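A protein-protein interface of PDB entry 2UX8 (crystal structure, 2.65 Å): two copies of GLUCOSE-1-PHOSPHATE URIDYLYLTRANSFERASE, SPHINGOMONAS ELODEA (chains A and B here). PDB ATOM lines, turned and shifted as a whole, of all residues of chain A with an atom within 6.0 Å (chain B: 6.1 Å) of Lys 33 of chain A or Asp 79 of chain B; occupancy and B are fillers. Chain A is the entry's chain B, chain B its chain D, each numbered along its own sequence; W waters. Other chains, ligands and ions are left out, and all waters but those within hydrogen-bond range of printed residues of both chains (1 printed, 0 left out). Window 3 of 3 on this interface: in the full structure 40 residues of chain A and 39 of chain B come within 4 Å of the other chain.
NZ of Lys 33 of chain A lies within hydrogen-bond range of OG1 of Thr 101 of chain B (2.7 Å). O of His 77 of chain B lies within hydrogen-bond range of NZ of Lys 33 of chain A (3.1 Å). The backbone carbonyl oxygen (O) of Asp 79 of chain B lies within hydrogen-bond range of the side-chain amino group (NZ) of Lys 33 of chain A (3.0 Å).
O of Leu 98 of chain B lies within hydrogen-bond range of OG1 of Thr 101 of chain B, at 2.5 Å. N of Ala 81 of chain B is in hydrogen-bond range of OE2 of Glu 85 of chain B (3.2 Å).
Among the printed residues, pairs that only touch across the chains: Pro 30 of chain A with His 77 of chain B, Pro 30 of chain A with Thr 101 of chain B, Lys 33 of chain A with Ala 81 of chain B, Ala 34 of chain A with Asp 76 of chain B and Ala 34 of chain A with His 77 of chain B.
Lys 33 of chain A touches four residues of chain B. Of the printed residues of chain A, Asp 76 of chain B touches Ala 34 (3.8 Å). Of the printed residues of chain A, Thr 101 of chain B touches Pro 30 (3.8 Å) and Lys 33 (2.7 Å). The nearest residue of chain B that does not touch Lys 33 of chain A is Leu 84 of chain B (4.1 Å). The nearest printed residue of chain B that does not touch Ala 34 of chain A is Leu 84 of chain B (5.9 Å).
Printed residues of chain A that touch a printed residue of chain B: Pro 30, Lys 33 and Ala 34. Hydrophobic or aromatic side chains of chain A within 4 Å of the printed part of chain B: Pro 30 and Ala 34. Of the 13 printed residues of chain B, 5 touch a printed residue of chain A. Along chain B the printed residues that touch a printed residue of chain A span positions 76 to 101. Among the printed residues, no Asp or Glu carboxylate lies within 4 Å of a Lys or Arg side-chain nitrogen of the other chain.
No position is printed for both chains.
Water W1 lies within hydrogen-bond range of the backbone NH of Ala 34 of chain A (2.7 Å), the backbone carbonyl oxygen of Ala 31 of chain A (2.8 Å), a ring nitrogen (ND1) of His 77 of chain B (2.9 Å), the backbone NH of Lys 33 of chain A (3.1 Å) and the backbone carbonyl oxygen of Pro 30 of chain A (3.3 Å).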
ATOM      1  N   PHE A  28      13.277 -16.043  12.511  1.00  0.00           N
ATOM      2  CA  PHE A  28      12.528 -17.288  12.645  1.00  0.00           C
ATOM      3  C   PHE A  28      11.194 -17.168  13.366  1.00  0.00           C
ATOM      4  O   PHE A  28      10.670 -18.155  13.883  1.00  0.00           O
ATOM      5  CB  PHE A  28      13.383 -18.354  13.345  1.00  0.00           C
ATOM      6  CG  PHE A  28      14.237 -19.158  12.410  1.00  0.00           C
ATOM      7  CD1 PHE A  28      15.333 -18.589  11.776  1.00  0.00           C
ATOM      8  CD2 PHE A  28      13.946 -20.492  12.169  1.00  0.00           C
ATOM      9  CE1 PHE A  28      16.136 -19.343  10.912  1.00  0.00           C
ATOM     10  CE2 PHE A  28      14.735 -21.257  11.314  1.00  0.00           C
ATOM     11  CZ  PHE A  28      15.835 -20.680  10.683  1.00  0.00           C
ATOM     12  N   LEU A  29      10.645 -15.962  13.411  1.00  0.00           N
ATOM     13  CA  LEU A  29       9.361 -15.749  14.065  1.00  0.00           C
ATOM     14  C   LEU A  29       8.294 -16.477  13.243  1.00  0.00           C
ATOM     15  O   LEU A  29       8.396 -16.576  12.028  1.00  0.00           O
ATOM     16  CB  LEU A  29       9.070 -14.240  14.149  1.00  0.00           C
ATOM     17  CG  LEU A  29       9.996 -13.487  15.124  1.00  0.00           C
ATOM     18  CD1 LEU A  29       9.783 -11.999  15.066  1.00  0.00           C
ATOM     19  CD2 LEU A  29       9.729 -13.982  16.521  1.00  0.00           C
ATOM     20  N   PRO A  30       7.239 -16.968  13.903  1.00  0.00           N
ATOM     21  CA  PRO A  30       6.991 -16.841  15.343  1.00  0.00           C
ATOM     22  C   PRO A  30       7.626 -17.917  16.224  1.00  0.00           C
ATOM     23  O   PRO A  30       7.400 -17.932  17.447  1.00  0.00           O
ATOM     24  CB  PRO A  30       5.470 -16.900  15.449  1.00  0.00           C
ATOM     25  CG  PRO A  30       4.969 -16.850  14.030  1.00  0.00           C
ATOM     26  CD  PRO A  30       6.038 -17.462  13.217  1.00  0.00           C
ATOM     27  N   ALA A  31       8.410 -18.806  15.625  1.00  0.00           N
ATOM     28  CA  ALA A  31       9.016 -19.894  16.379  1.00  0.00           C
ATOM     29  C   ALA A  31       9.902 -19.395  17.504  1.00  0.00           C
ATOM     30  O   ALA A  31       9.948 -19.980  18.585  1.00  0.00           O
ATOM     31  CB  ALA A  31       9.819 -20.810  15.451  1.00  0.00           C
ATOM     32  N   THR A  32      10.608 -18.307  17.255  1.00  0.00           N
ATOM     33  CA  THR A  32      11.499 -17.781  18.264  1.00  0.00           C
ATOM     34  C   THR A  32      10.905 -16.647  19.091  1.00  0.00           C
ATOM     35  O   THR A  32      11.634 -15.887  19.724  1.00  0.00           O
ATOM     36  CB  THR A  32      12.808 -17.306  17.628  1.00  0.00           C
ATOM     37  OG1 THR A  32      12.507 -16.465  16.514  1.00  0.00           O
ATOM     38  CG2 THR A  32      13.633 -18.482  17.150  1.00  0.00           C
ATOM     39  N   LYS A  33       9.582 -16.539  19.106  1.00  0.00           N
ATOM     40  CA  LYS A  33       8.936 -15.487  19.874  1.00  0.00           C
ATOM     41  C   LYS A  33       9.152 -15.656  21.379  1.00  0.00           C
ATOM     42  O   LYS A  33       9.309 -14.680  22.104  1.00  0.00           O
ATOM     43  CB  LYS A  33       7.437 -15.463  19.576  1.00  0.00           C
ATOM     44  CG  LYS A  33       6.652 -14.454  20.406  1.00  0.00           C
ATOM     45  CD  LYS A  33       5.155 -14.547  20.154  1.00  0.00           C
ATOM     46  CE  LYS A  33       4.404 -13.592  21.067  1.00  0.00           C
ATOM     47  NZ  LYS A  33       2.939 -13.552  20.819  1.00  0.00           N
ATOM     48  N   ALA A  34       9.156 -16.893  21.854  1.00  0.00           N
ATOM     49  CA  ALA A  34       9.341 -17.130  23.276  1.00  0.00           C
ATOM     50  C   ALA A  34      10.337 -18.236  23.519  1.00  0.00           C
ATOM     51  O   ALA A  34      10.396 -18.785  24.612  1.00  0.00           O
ATOM     52  CB  ALA A  34       8.002 -17.465  23.954  1.00  0.00           C
ATOM     53  N   MET A  35      11.100 -18.596  22.496  1.00  0.00           N
ATOM     54  CA  MET A  35      12.109 -19.611  22.688  1.00  0.00           C
ATOM     55  C   MET A  35      13.362 -19.209  21.962  1.00  0.00           C
ATOM     56  O   MET A  35      13.311 -18.704  20.844  1.00  0.00           O
ATOM     57  CB  MET A  35      11.612 -20.990  22.271  1.00  0.00           C
ATOM     58  CG  MET A  35      10.744 -21.604  23.358  1.00  0.00           C
ATOM     59  SD  MET A  35      11.075 -23.354  23.605  1.00  0.00           S
ATOM     60  CE  MET A  35      12.592 -23.287  24.478  1.00  0.00           C
ATOM     61  N   GLU B  75       3.398 -20.730  27.738  1.00  0.00           N
ATOM     62  CA  GLU B  75       2.572 -19.655  28.256  1.00  0.00           C
ATOM     63  C   GLU B  75       3.025 -18.302  27.720  1.00  0.00           C
ATOM     64  O   GLU B  75       2.203 -17.455  27.400  1.00  0.00           O
ATOM     65  CB  GLU B  75       2.609 -19.671  29.778  1.00  0.00           C
ATOM     66  CG  GLU B  75       1.274 -19.395  30.429  1.00  0.00           C
ATOM     67  CD  GLU B  75       1.290 -19.687  31.921  1.00  0.00           C
ATOM     68  OE1 GLU B  75       1.697 -20.809  32.302  1.00  0.00           O
ATOM     69  OE2 GLU B  75       0.893 -18.798  32.710  1.00  0.00           O
ATOM     70  N   ASP B  76       4.330 -18.103  27.609  1.00  0.00           N
ATOM     71  CA  ASP B  76       4.844 -16.843  27.100  1.00  0.00           C
ATOM     72  C   ASP B  76       4.579 -16.690  25.612  1.00  0.00           C
ATOM     73  O   ASP B  76       4.346 -15.578  25.120  1.00  0.00           O
ATOM     74  CB  ASP B  76       6.346 -16.720  27.338  1.00  0.00           C
ATOM     75  CG  ASP B  76       6.687 -16.560  28.788  1.00  0.00           C
ATOM     76  OD1 ASP B  76       5.893 -15.927  29.514  1.00  0.00           O
ATOM     77  OD2 ASP B  76       7.756 -17.061  29.193  1.00  0.00           O
ATOM     78  N   HIS B  77       4.618 -17.802  24.886  1.00  0.00           N
ATOM     79  CA  HIS B  77       4.394 -17.727  23.455  1.00  0.00           C
ATOM     80  C   HIS B  77       3.053 -17.089  23.124  1.00  0.00           C
ATOM     81  O   HIS B  77       2.927 -16.408  22.117  1.00  0.00           O
ATOM     82  CB  HIS B  77       4.452 -19.108  22.804  1.00  0.00           C
ATOM     83  CG  HIS B  77       4.235 -19.071  21.320  1.00  0.00           C
ATOM     84  ND1 HIS B  77       5.252 -18.821  20.423  1.00  0.00           N
ATOM     85  CD2 HIS B  77       3.100 -19.154  20.584  1.00  0.00           C
ATOM     86  CE1 HIS B  77       4.754 -18.746  19.202  1.00  0.00           C
ATOM     87  NE2 HIS B  77       3.451 -18.943  19.273  1.00  0.00           N
ATOM     88  N   PHE B  78       2.052 -17.304  23.970  1.00  0.00           N
ATOM     89  CA  PHE B  78       0.732 -16.747  23.706  1.00  0.00           C
ATOM     90  C   PHE B  78       0.381 -15.492  24.464  1.00  0.00           C
ATOM     91  O   PHE B  78      -0.788 -15.223  24.726  1.00  0.00           O
ATOM     92  CB  PHE B  78      -0.344 -17.806  23.935  1.00  0.00           C
ATOM     93  CG  PHE B  78      -0.276 -18.930  22.960  1.00  0.00           C
ATOM     94  CD1 PHE B  78       0.440 -20.086  23.260  1.00  0.00           C
ATOM     95  CD2 PHE B  78      -0.862 -18.807  21.706  1.00  0.00           C
ATOM     96  CE1 PHE B  78       0.577 -21.109  22.317  1.00  0.00           C
ATOM     97  CE2 PHE B  78      -0.732 -19.822  20.753  1.00  0.00           C
ATOM     98  CZ  PHE B  78      -0.011 -20.975  21.059  1.00  0.00           C
ATOM     99  N   ASP B  79       1.396 -14.723  24.828  1.00  0.00           N
ATOM    100  CA  ASP B  79       1.171 -13.467  25.522  1.00  0.00           C
ATOM    101  C   ASP B  79       1.970 -12.442  24.737  1.00  0.00           C
ATOM    102  O   ASP B  79       2.606 -12.775  23.734  1.00  0.00           O
ATOM    103  CB  ASP B  79       1.666 -13.531  26.975  1.00  0.00           C
ATOM    104  CG  ASP B  79       1.127 -12.382  27.841  1.00  0.00           C
ATOM    105  OD1 ASP B  79       0.448 -11.477  27.310  1.00  0.00           O
ATOM    106  OD2 ASP B  79       1.383 -12.380  29.064  1.00  0.00           O
ATOM    107  N   ILE B  80       1.915 -11.190  25.172  1.00  0.00           N
ATOM    108  CA  ILE B  80       2.658 -10.133  24.517  1.00  0.00           C
ATOM    109  C   ILE B  80       4.127 -10.325  24.848  1.00  0.00           C
ATOM    110  O   ILE B  80       4.492 -10.501  26.011  1.00  0.00           O
ATOM    111  CB  ILE B  80       2.241  -8.756  25.047  1.00  0.00           C
ATOM    112  CG1 ILE B  80       0.796  -8.460  24.677  1.00  0.00           C
ATOM    113  CG2 ILE B  80       3.171  -7.691  24.502  1.00  0.00           C
ATOM    114  CD1 ILE B  80       0.324  -7.141  25.212  1.00  0.00           C
ATOM    115  N   ALA B  81       4.963 -10.304  23.820  1.00  0.00           N
ATOM    116  CA  ALA B  81       6.399 -10.435  23.999  1.00  0.00           C
ATOM    117  C   ALA B  81       6.913  -8.985  24.041  1.00  0.00           C
ATOM    118  O   ALA B  81       7.480  -8.472  23.071  1.00  0.00           O
ATOM    119  CB  ALA B  81       6.990 -11.198  22.819  1.00  0.00           C
ATOM    120  N   LEU B  84      10.533  -7.761  22.751  1.00  0.00           N
ATOM    121  CA  LEU B  84      10.679  -8.091  21.344  1.00  0.00           C
ATOM    122  C   LEU B  84       9.915  -7.123  20.452  1.00  0.00           C
ATOM    123  O   LEU B  84      10.492  -6.527  19.553  1.00  0.00           O
ATOM    124  CB  LEU B  84      10.180  -9.514  21.105  1.00  0.00           C
ATOM    125  CG  LEU B  84      10.054 -10.030  19.671  1.00  0.00           C
ATOM    126  CD1 LEU B  84      11.425 -10.190  19.037  1.00  0.00           C
ATOM    127  CD2 LEU B  84       9.340 -11.353  19.697  1.00  0.00           C
ATOM    128  N   GLU B  85       8.619  -6.977  20.716  1.00  0.00           N
ATOM    129  CA  GLU B  85       7.763  -6.107  19.931  1.00  0.00           C
ATOM    130  C   GLU B  85       8.237  -4.660  19.953  1.00  0.00           C
ATOM    131  O   GLU B  85       8.055  -3.916  18.984  1.00  0.00           O
ATOM    132  CB  GLU B  85       6.327  -6.256  20.432  1.00  0.00           C
ATOM    133  CG  GLU B  85       5.811  -7.663  20.189  1.00  0.00           C
ATOM    134  CD  GLU B  85       4.389  -7.885  20.641  1.00  0.00           C
ATOM    135  OE1 GLU B  85       3.571  -6.942  20.554  1.00  0.00           O
ATOM    136  OE2 GLU B  85       4.081  -9.020  21.065  1.00  0.00           O
ATOM    137  N   LEU B  98       3.580 -11.968  13.843  1.00  0.00           N
ATOM    138  CA  LEU B  98       3.102 -12.492  15.107  1.00  0.00           C
ATOM    139  C   LEU B  98       1.595 -12.586  15.178  1.00  0.00           C
ATOM    140  O   LEU B  98       1.045 -12.934  16.216  1.00  0.00           O
ATOM    141  CB  LEU B  98       3.599 -11.615  16.254  1.00  0.00           C
ATOM    142  CG  LEU B  98       5.097 -11.310  16.343  1.00  0.00           C
ATOM    143  CD1 LEU B  98       5.321 -10.384  17.514  1.00  0.00           C
ATOM    144  CD2 LEU B  98       5.904 -12.591  16.518  1.00  0.00           C
ATOM    145  N   THR B 101      -0.593 -15.154  17.290  1.00  0.00           N
ATOM    146  CA  THR B 101       0.162 -15.670  18.423  1.00  0.00           C
ATOM    147  C   THR B 101      -0.430 -15.206  19.744  1.00  0.00           C
ATOM    148  O   THR B 101      -0.076 -15.713  20.815  1.00  0.00           O
ATOM    149  CB  THR B 101       1.641 -15.254  18.391  1.00  0.00           C
ATOM    150  OG1 THR B 101       1.737 -13.837  18.435  1.00  0.00           O
ATOM    151  CG2 THR B 101       2.315 -15.750  17.146  1.00  0.00           C
ATOM    152  N   ARG B 102      -1.342 -14.247  19.669  1.00  0.00           N
ATOM    153  CA  ARG B 102      -1.980 -13.732  20.866  1.00  0.00           C
ATOM    154  C   ARG B 102      -3.488 -13.670  20.690  1.00  0.00           C
ATOM    155  O   ARG B 102      -3.985 -13.102  19.729  1.00  0.00           O
ATOM    156  CB  ARG B 102      -1.418 -12.350  21.184  1.00  0.00           C
ATOM    157  CG  ARG B 102      -2.115 -11.633  22.307  1.00  0.00           C
ATOM    158  CD  ARG B 102      -1.269 -10.493  22.844  1.00  0.00           C
ATOM    159  NE  ARG B 102      -0.950  -9.511  21.819  1.00  0.00           N
ATOM    160  CZ  ARG B 102      -1.477  -8.294  21.756  1.00  0.00           C
ATOM    161  NH1 ARG B 102      -2.354  -7.900  22.668  1.00  0.00           N
ATOM    162  NH2 ARG B 102      -1.130  -7.473  20.772  1.00  0.00           N
ATOM    163  N   TYR B 110      -4.772 -21.998  31.576  1.00  0.00           N
ATOM    164  CA  TYR B 110      -3.810 -23.033  31.883  1.00  0.00           C
ATOM    165  C   TYR B 110      -4.106 -23.682  33.233  1.00  0.00           C
ATOM    166  O   TYR B 110      -4.495 -23.007  34.194  1.00  0.00           O
ATOM    167  CB  TYR B 110      -2.400 -22.448  31.905  1.00  0.00           C
ATOM    168  CG  TYR B 110      -1.991 -21.708  30.655  1.00  0.00           C
ATOM    169  CD1 TYR B 110      -2.486 -20.436  30.374  1.00  0.00           C
ATOM    170  CD2 TYR B 110      -1.067 -22.262  29.774  1.00  0.00           C
ATOM    171  CE1 TYR B 110      -2.062 -19.732  29.242  1.00  0.00           C
ATOM    172  CE2 TYR B 110      -0.636 -21.576  28.643  1.00  0.00           C
ATOM    173  CZ  TYR B 110      -1.131 -20.313  28.381  1.00  0.00           C
ATOM    174  OH  TYR B 110      -0.671 -19.636  27.268  1.00  0.00           O
HETATM  175  O   HOH W   1       8.156 -18.944  20.497  1.00  0.00           O
